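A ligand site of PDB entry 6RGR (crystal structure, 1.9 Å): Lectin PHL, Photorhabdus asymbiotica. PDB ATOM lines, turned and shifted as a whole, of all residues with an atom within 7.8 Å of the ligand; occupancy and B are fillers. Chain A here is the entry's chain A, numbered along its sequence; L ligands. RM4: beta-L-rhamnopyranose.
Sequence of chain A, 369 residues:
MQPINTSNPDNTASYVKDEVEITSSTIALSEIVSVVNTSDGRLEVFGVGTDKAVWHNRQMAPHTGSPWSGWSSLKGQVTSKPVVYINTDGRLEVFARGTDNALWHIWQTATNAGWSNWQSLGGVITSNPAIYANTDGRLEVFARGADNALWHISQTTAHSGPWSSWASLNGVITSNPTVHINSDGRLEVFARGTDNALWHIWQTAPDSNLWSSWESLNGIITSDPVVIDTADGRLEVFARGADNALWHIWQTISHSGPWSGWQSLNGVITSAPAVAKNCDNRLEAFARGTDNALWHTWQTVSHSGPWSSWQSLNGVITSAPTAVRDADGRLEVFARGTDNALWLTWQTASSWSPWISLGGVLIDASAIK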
ATOM      1  N   ASN A 182      -2.203   2.362  18.567  1.00  0.00           N
ATOM      2  CA  ASN A 182      -2.683   2.419  19.968  1.00  0.00           C
ATOM      3  C   ASN A 182      -3.863   1.467  20.145  1.00  0.00           C
ATOM      4  O   ASN A 182      -4.499   1.070  19.123  1.00  0.00           O
ATOM      5  CB  ASN A 182      -3.006   3.851  20.383  1.00  0.00           C
ATOM      6  CG  ASN A 182      -1.755   4.636  20.703  1.00  0.00           C
ATOM      7  OD1 ASN A 182      -1.236   4.532  21.818  1.00  0.00           O
ATOM      8  ND2 ASN A 182      -1.264   5.387  19.731  1.00  0.00           N
ATOM      9  N   ASP A 184      -6.597   2.164  21.176  1.00  0.00           N
ATOM     10  CA  ASP A 184      -7.811   2.914  20.759  1.00  0.00           C
ATOM     11  C   ASP A 184      -7.829   3.153  19.230  1.00  0.00           C
ATOM     12  O   ASP A 184      -8.672   3.957  18.809  1.00  0.00           O
ATOM     13  CB  ASP A 184      -7.918   4.235  21.527  1.00  0.00           C
ATOM     14  CG  ASP A 184      -6.780   5.206  21.224  1.00  0.00           C
ATOM     15  OD1 ASP A 184      -5.910   4.880  20.391  1.00  0.00           O
ATOM     16  OD2 ASP A 184      -6.798   6.288  21.809  1.00  0.00           O
ATOM     17  N   ARG A 186      -5.530   4.568  17.165  1.00  0.00           N
ATOM     18  CA  ARG A 186      -4.733   5.707  16.636  1.00  0.00           C
ATOM     19  C   ARG A 186      -3.323   5.216  16.275  1.00  0.00           C
ATOM     20  O   ARG A 186      -2.631   4.666  17.141  1.00  0.00           O
ATOM     21  CB  ARG A 186      -4.673   6.865  17.642  1.00  0.00           C
ATOM     22  CG  ARG A 186      -6.009   7.506  17.967  1.00  0.00           C
ATOM     23  CD  ARG A 186      -5.934   8.572  19.045  1.00  0.00           C
ATOM     24  NE  ARG A 186      -5.370   8.021  20.269  1.00  0.00           N
ATOM     25  CZ  ARG A 186      -4.092   8.120  20.651  1.00  0.00           C
ATOM     26  NH1 ARG A 186      -3.219   8.817  19.944  1.00  0.00           N
ATOM     27  NH2 ARG A 186      -3.697   7.527  21.762  1.00  0.00           N
ATOM     28  N   LEU A 187      -2.912   5.422  15.015  1.00  0.00           N
ATOM     29  CA  LEU A 187      -1.518   5.183  14.552  1.00  0.00           C
ATOM     30  C   LEU A 187      -0.584   6.157  15.268  1.00  0.00           C
ATOM     31  O   LEU A 187      -1.020   7.292  15.609  1.00  0.00           O
ATOM     32  CB  LEU A 187      -1.436   5.350  13.037  1.00  0.00           C
ATOM     33  CG  LEU A 187      -2.261   4.354  12.218  1.00  0.00           C
ATOM     34  CD1 LEU A 187      -1.979   4.524  10.736  1.00  0.00           C
ATOM     35  CD2 LEU A 187      -2.011   2.914  12.669  1.00  0.00           C
ATOM     36  N   GLU A 188       0.631   5.697  15.552  1.00  0.00           N
ATOM     37  CA  GLU A 188       1.706   6.475  16.204  1.00  0.00           C
ATOM     38  C   GLU A 188       3.050   6.119  15.556  1.00  0.00           C
ATOM     39  O   GLU A 188       3.336   4.912  15.384  1.00  0.00           O
ATOM     40  CB  GLU A 188       1.709   6.203  17.705  1.00  0.00           C
ATOM     41  CG  GLU A 188       2.568   7.177  18.503  1.00  0.00           C
ATOM     42  CD  GLU A 188       2.158   7.306  19.963  1.00  0.00           C
ATOM     43  OE1 GLU A 188       1.014   6.936  20.296  1.00  0.00           O
ATOM     44  OE2 GLU A 188       2.978   7.807  20.759  1.00  0.00           O
ATOM     45  N   VAL A 189       3.828   7.137  15.199  1.00  0.00           N
ATOM     46  CA  VAL A 189       5.120   6.955  14.489  1.00  0.00           C
ATOM     47  C   VAL A 189       6.251   7.466  15.384  1.00  0.00           C
ATOM     48  O   VAL A 189       6.091   8.565  16.003  1.00  0.00           O
ATOM     49  CB  VAL A 189       5.128   7.637  13.117  1.00  0.00           C
ATOM     50  CG1 VAL A 189       6.447   7.425  12.397  1.00  0.00           C
ATOM     51  CG2 VAL A 189       3.952   7.165  12.274  1.00  0.00           C
ATOM     52  N   PHE A 190       7.325   6.692  15.411  1.00  0.00           N
ATOM     53  CA  PHE A 190       8.569   6.934  16.186  1.00  0.00           C
ATOM     54  C   PHE A 190       9.765   7.043  15.231  1.00  0.00           C
ATOM     55  O   PHE A 190       9.838   6.277  14.251  1.00  0.00           O
ATOM     56  CB  PHE A 190       8.752   5.810  17.205  1.00  0.00           C
ATOM     57  CG  PHE A 190       7.587   5.657  18.139  1.00  0.00           C
ATOM     58  CD1 PHE A 190       6.464   4.932  17.763  1.00  0.00           C
ATOM     59  CD2 PHE A 190       7.608   6.254  19.381  1.00  0.00           C
ATOM     60  CE1 PHE A 190       5.383   4.804  18.623  1.00  0.00           C
ATOM     61  CE2 PHE A 190       6.534   6.130  20.248  1.00  0.00           C
ATOM     62  CZ  PHE A 190       5.418   5.404  19.865  1.00  0.00           C
ATOM     63  N   HIS A 200       8.145  11.373  18.509  1.00  0.00           N
ATOM     64  CA  HIS A 200       6.929  10.666  18.038  1.00  0.00           C
ATOM     65  C   HIS A 200       5.840  11.658  17.652  1.00  0.00           C
ATOM     66  O   HIS A 200       5.887  12.845  18.089  1.00  0.00           O
ATOM     67  CB  HIS A 200       6.472   9.608  19.062  1.00  0.00           C
ATOM     68  CG  HIS A 200       6.040  10.148  20.383  1.00  0.00           C
ATOM     69  ND1 HIS A 200       4.963   9.614  21.085  1.00  0.00           N
ATOM     70  CD2 HIS A 200       6.536  11.145  21.157  1.00  0.00           C
ATOM     71  CE1 HIS A 200       4.811  10.273  22.213  1.00  0.00           C
ATOM     72  NE2 HIS A 200       5.774  11.220  22.291  1.00  0.00           N
ATOM     73  N   ILE A 201       4.897  11.160  16.867  1.00  0.00           N
ATOM     74  CA  ILE A 201       3.691  11.881  16.385  1.00  0.00           C
ATOM     75  C   ILE A 201       2.578  10.826  16.250  1.00  0.00           C
ATOM     76  O   ILE A 201       2.914   9.636  15.997  1.00  0.00           O
ATOM     77  CB  ILE A 201       4.028  12.597  15.070  1.00  0.00           C
ATOM     78  CG1 ILE A 201       2.927  13.583  14.670  1.00  0.00           C
ATOM     79  CG2 ILE A 201       4.365  11.604  13.987  1.00  0.00           C
ATOM     80  CD1 ILE A 201       3.302  14.488  13.505  1.00  0.00           C
ATOM     81  N   TRP A 202       1.327  11.228  16.466  1.00  0.00           N
ATOM     82  CA  TRP A 202       0.187  10.278  16.520  1.00  0.00           C
ATOM     83  C   TRP A 202      -1.037  10.864  15.846  1.00  0.00           C
ATOM     84  O   TRP A 202      -1.214  12.098  15.866  1.00  0.00           O
ATOM     85  CB  TRP A 202      -0.106   9.833  17.969  1.00  0.00           C
ATOM     86  CG  TRP A 202      -0.318  10.952  18.940  1.00  0.00           C
ATOM     87  CD1 TRP A 202      -1.493  11.533  19.319  1.00  0.00           C
ATOM     88  CD2 TRP A 202       0.718  11.612  19.680  1.00  0.00           C
ATOM     89  NE1 TRP A 202      -1.261  12.519  20.249  1.00  0.00           N
ATOM     90  CE2 TRP A 202       0.084  12.596  20.481  1.00  0.00           C
ATOM     91  CE3 TRP A 202       2.114  11.501  19.713  1.00  0.00           C
ATOM     92  CZ2 TRP A 202       0.810  13.425  21.338  1.00  0.00           C
ATOM     93  CZ3 TRP A 202       2.820  12.321  20.548  1.00  0.00           C
ATOM     94  CH2 TRP A 202       2.171  13.270  21.350  1.00  0.00           C
ATOM     95  N   GLN A 203      -1.889   9.996  15.292  1.00  0.00           N
ATOM     96  CA  GLN A 203      -3.265  10.376  14.905  1.00  0.00           C
ATOM     97  C   GLN A 203      -3.999  10.851  16.158  1.00  0.00           C
ATOM     98  O   GLN A 203      -3.732  10.300  17.237  1.00  0.00           O
ATOM     99  CB  GLN A 203      -4.015   9.215  14.265  1.00  0.00           C
ATOM    100  CG  GLN A 203      -3.507   8.860  12.877  1.00  0.00           C
ATOM    101  CD  GLN A 203      -4.202   7.610  12.371  1.00  0.00           C
ATOM    102  OE1 GLN A 203      -4.614   6.749  13.137  1.00  0.00           O
ATOM    103  NE2 GLN A 203      -4.300   7.508  11.056  1.00  0.00           N
ATOM    104  N   THR A 204      -4.866  11.843  16.028  1.00  0.00           N
ATOM    105  CA  THR A 204      -5.727  12.330  17.148  1.00  0.00           C
ATOM    106  C   THR A 204      -7.057  11.559  17.134  1.00  0.00           C
ATOM    107  O   THR A 204      -7.769  11.664  18.125  1.00  0.00           O
ATOM    108  CB  THR A 204      -5.906  13.855  17.078  1.00  0.00           C
ATOM    109  OG1 THR A 204      -6.521  14.188  15.829  1.00  0.00           O
ATOM    110  CG2 THR A 204      -4.585  14.569  17.224  1.00  0.00           C
ATOM    111  N   SER A 212      -1.099  14.922  15.787  1.00  0.00           N
ATOM    112  CA  SER A 212      -0.473  15.743  16.851  1.00  0.00           C
ATOM    113  C   SER A 212       0.716  16.499  16.259  1.00  0.00           C
ATOM    114  O   SER A 212       1.128  16.182  15.124  1.00  0.00           O
ATOM    115  CB  SER A 212      -0.017  14.870  17.980  1.00  0.00           C
ATOM    116  OG  SER A 212       1.074  14.054  17.571  1.00  0.00           O
ATOM    117  N   GLU A 215       6.565  15.344  19.244  1.00  0.00           N
ATOM    118  CA  GLU A 215       6.985  15.520  20.649  1.00  0.00           C
ATOM    119  C   GLU A 215       8.229  14.683  20.894  1.00  0.00           C
ATOM    120  O   GLU A 215       8.379  13.637  20.244  1.00  0.00           O
ATOM    121  CB  GLU A 215       5.870  15.168  21.628  1.00  0.00           C
ATOM    122  CG  GLU A 215       4.763  16.213  21.676  1.00  0.00           C
ATOM    123  CD  GLU A 215       3.892  16.196  22.922  1.00  0.00           C
ATOM    124  OE1 GLU A 215       4.160  15.365  23.844  1.00  0.00           O
ATOM    125  OE2 GLU A 215       2.938  17.003  22.969  1.00  0.00           O
ATOM    126  N   LEU A 217      10.619  12.292  23.267  1.00  0.00           N
ATOM    127  CA  LEU A 217      10.694  11.368  24.419  1.00  0.00           C
ATOM    128  C   LEU A 217      12.143  11.372  24.947  1.00  0.00           C
ATOM    129  O   LEU A 217      12.479  10.472  25.740  1.00  0.00           O
ATOM    130  CB  LEU A 217      10.248   9.973  23.983  1.00  0.00           C
ATOM    131  CG  LEU A 217       8.752   9.816  23.752  1.00  0.00           C
ATOM    132  CD1 LEU A 217       8.430   8.428  23.230  1.00  0.00           C
ATOM    133  CD2 LEU A 217       7.967  10.098  25.025  1.00  0.00           C
ATOM    134  N   LEU A 235       1.958   1.054  24.180  1.00  0.00           N
ATOM    135  CA  LEU A 235       3.150   1.055  23.292  1.00  0.00           C
ATOM    136  C   LEU A 235       4.392   1.095  24.174  1.00  0.00           C
ATOM    137  O   LEU A 235       4.414   1.889  25.154  1.00  0.00           O
ATOM    138  CB  LEU A 235       3.098   2.239  22.326  1.00  0.00           C
ATOM    139  CG  LEU A 235       1.915   2.246  21.354  1.00  0.00           C
ATOM    140  CD1 LEU A 235       2.057   3.397  20.371  1.00  0.00           C
ATOM    141  CD2 LEU A 235       1.785   0.908  20.636  1.00  0.00           C
ATOM    142  N   TRP A 250       7.883   3.431  27.820  1.00  0.00           N
ATOM    143  CA  TRP A 250       6.505   2.927  27.558  1.00  0.00           C
ATOM    144  C   TRP A 250       5.447   3.940  28.002  1.00  0.00           C
ATOM    145  O   TRP A 250       5.717   4.768  28.914  1.00  0.00           O
ATOM    146  CB  TRP A 250       6.316   1.588  28.258  1.00  0.00           C
ATOM    147  CG  TRP A 250       6.576   1.640  29.734  1.00  0.00           C
ATOM    148  CD1 TRP A 250       5.684   1.973  30.710  1.00  0.00           C
ATOM    149  CD2 TRP A 250       7.816   1.351  30.399  1.00  0.00           C
ATOM    150  NE1 TRP A 250       6.278   1.907  31.940  1.00  0.00           N
ATOM    151  CE2 TRP A 250       7.583   1.512  31.786  1.00  0.00           C
ATOM    152  CE3 TRP A 250       9.088   0.955  29.977  1.00  0.00           C
ATOM    153  CZ2 TRP A 250       8.579   1.318  32.742  1.00  0.00           C
ATOM    154  CZ3 TRP A 250      10.072   0.746  30.922  1.00  0.00           C
ATOM    155  CH2 TRP A 250       9.820   0.937  32.283  1.00  0.00           C
ATOM    156  N   GLN A 251       4.271   3.847  27.369  1.00  0.00           N
ATOM    157  CA  GLN A 251       3.045   4.573  27.769  1.00  0.00           C
ATOM    158  C   GLN A 251       2.598   4.080  29.151  1.00  0.00           C
ATOM    159  O   GLN A 251       2.798   2.891  29.446  1.00  0.00           O
ATOM    160  CB  GLN A 251       1.950   4.320  26.724  1.00  0.00           C
ATOM    161  CG  GLN A 251       2.178   5.012  25.391  1.00  0.00           C
ATOM    162  CD  GLN A 251       1.063   4.656  24.440  1.00  0.00           C
ATOM    163  OE1 GLN A 251       0.437   3.606  24.561  1.00  0.00           O
ATOM    164  NE2 GLN A 251       0.799   5.546  23.501  1.00  0.00           N
ATOM    165  N   THR A 252       1.979   4.948  29.949  1.00  0.00           N
ATOM    166  CA  THR A 252       1.525   4.646  31.335  1.00  0.00           C
ATOM    167  C   THR A 252       0.088   4.097  31.316  1.00  0.00           C
ATOM    168  O   THR A 252      -0.563   4.277  30.285  1.00  0.00           O
ATOM    169  CB  THR A 252       1.676   5.874  32.241  1.00  0.00           C
ATOM    170  OG1 THR A 252       1.021   6.978  31.613  1.00  0.00           O
ATOM    171  CG2 THR A 252       3.128   6.209  32.529  1.00  0.00           C
ATOM    172  N   SER A 256      -4.666   8.175  28.704  1.00  0.00           N
ATOM    173  CA  SER A 256      -4.316   9.514  28.158  1.00  0.00           C
ATOM    174  C   SER A 256      -3.338  10.252  29.086  1.00  0.00           C
ATOM    175  O   SER A 256      -3.528  11.476  29.291  1.00  0.00           O
ATOM    176  CB  SER A 256      -5.564  10.329  27.912  1.00  0.00           C
ATOM    177  N   GLY A 257      -2.304   9.562  29.595  1.00  0.00           N
ATOM    178  CA  GLY A 257      -1.238  10.115  30.457  1.00  0.00           C
ATOM    179  C   GLY A 257       0.143  10.021  29.812  1.00  0.00           C
ATOM    180  O   GLY A 257       0.270   9.575  28.666  1.00  0.00           O
ATOM    181  N   PRO A 258       1.225  10.406  30.524  1.00  0.00           N
ATOM    182  CA  PRO A 258       2.573  10.512  29.930  1.00  0.00           C
ATOM    183  C   PRO A 258       3.346   9.189  29.857  1.00  0.00           C
ATOM    184  O   PRO A 258       2.893   8.207  30.388  1.00  0.00           O
ATOM    185  CB  PRO A 258       3.278  11.468  30.904  1.00  0.00           C
ATOM    186  CG  PRO A 258       2.687  11.096  32.246  1.00  0.00           C
ATOM    187  CD  PRO A 258       1.231  10.739  31.957  1.00  0.00           C
ATOM    188  N   TRP A 259       4.505   9.207  29.189  1.00  0.00           N
ATOM    189  CA  TRP A 259       5.390   8.016  29.067  1.00  0.00           C
ATOM    190  C   TRP A 259       6.204   7.845  30.347  1.00  0.00           C
ATOM    191  O   TRP A 259       6.301   8.813  31.122  1.00  0.00           O
ATOM    192  CB  TRP A 259       6.306   8.134  27.848  1.00  0.00           C
ATOM    193  CG  TRP A 259       5.581   7.915  26.554  1.00  0.00           C
ATOM    194  CD1 TRP A 259       4.608   8.706  26.029  1.00  0.00           C
ATOM    195  CD2 TRP A 259       5.758   6.824  25.631  1.00  0.00           C
ATOM    196  NE1 TRP A 259       4.172   8.198  24.835  1.00  0.00           N
ATOM    197  CE2 TRP A 259       4.855   7.044  24.566  1.00  0.00           C
ATOM    198  CE3 TRP A 259       6.591   5.702  25.595  1.00  0.00           C
ATOM    199  CZ2 TRP A 259       4.766   6.166  23.485  1.00  0.00           C
ATOM    200  CZ3 TRP A 259       6.498   4.847  24.523  1.00  0.00           C
ATOM    201  CH2 TRP A 259       5.599   5.078  23.491  1.00  0.00           C
HETATM  202  C1  RM4 L   1      -0.478   9.200  22.532  1.00  0.00           C
HETATM  203  C2  RM4 L   1       0.993   9.569  22.745  1.00  0.00           C
HETATM  204  C3  RM4 L   1       1.065  10.465  24.003  1.00  0.00           C
HETATM  205  C4  RM4 L   1       0.402   9.748  25.156  1.00  0.00           C
HETATM  206  C5  RM4 L   1      -1.018   9.249  24.829  1.00  0.00           C
HETATM  207  C6  RM4 L   1      -1.621   8.378  25.927  1.00  0.00           C
HETATM  208  O1  RM4 L   1      -0.645   8.367  21.402  1.00  0.00           O
HETATM  209  O2  RM4 L   1       1.800   8.392  22.929  1.00  0.00           O
HETATM  210  O3  RM4 L   1       2.426  10.734  24.374  1.00  0.00           O
HETATM  211  O4  RM4 L   1       0.383  10.663  26.246  1.00  0.00           O
HETATM  212  O5  RM4 L   1      -0.984   8.465  23.637  1.00  0.00           O
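Residues that only touch the ligand: His 200, Trp 202 and Ser 256.
Hydrophobic or aromatic side chains within 4 Å of the ligand: His 200, Trp 202 and Trp 259.
Of the 23 residues printed, 9 come within 4 Å of the ligand.
The nearest printed residue that does not touch the ligand is Pro 258 (4.3 Å).
OE2 of Glu 188 lies within hydrogen-bond range of ND1 of His 200.
The side-chain carboxylate (OE1) of Glu 188 is in hydrogen-bond range of the side-chain amide nitrogen (ND2) of Asn 182, 2.8 Å away.
The side-chain amide nitrogen (ND2) of Asn 182 lies within hydrogen-bond range of the backbone carbonyl oxygen (O) of Arg 186.
NH1 of Arg 186 is in hydrogen-bond range of O of Gln 203, at 3.1 Å.
NE of Arg 186 lies within salt-bridge range of OD2 of Asp 184 (2.7 Å).
The side-chain amide nitrogen (NE2) of Gln 251 lies within hydrogen-bond range of the side-chain amide oxygen (OD1) of Asn 182, at 2.8 Å.
The backbone NH (N) of Gln 251 lies within hydrogen-bond range of the backbone carbonyl oxygen (O) of Leu 235.
N of Glu 215 is in hydrogen-bond range of O of His 200 (2.8 Å).
The side-chain carboxylate (OE1) of Glu 188 lies within hydrogen-bond range of an oxygen (O1) of the ligand (2.5 Å).
The backbone carbonyl oxygen (O) of Gly 257 lies within hydrogen-bond range of an oxygen (O4) of the ligand, at 2.7 Å.
O1 of the ligand sits at hydrogen-bond distance from NH1 of Arg 186.
NE1 of Trp 259 lies within hydrogen-bond range of O2 of the ligand, 3.0 Å away.
An oxygen (O2) of the ligand is in hydrogen-bond range of the side-chain amide nitrogen of Gln 251.
O1 of the ligand is in hydrogen-bond range of ND2 of Asn 182.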
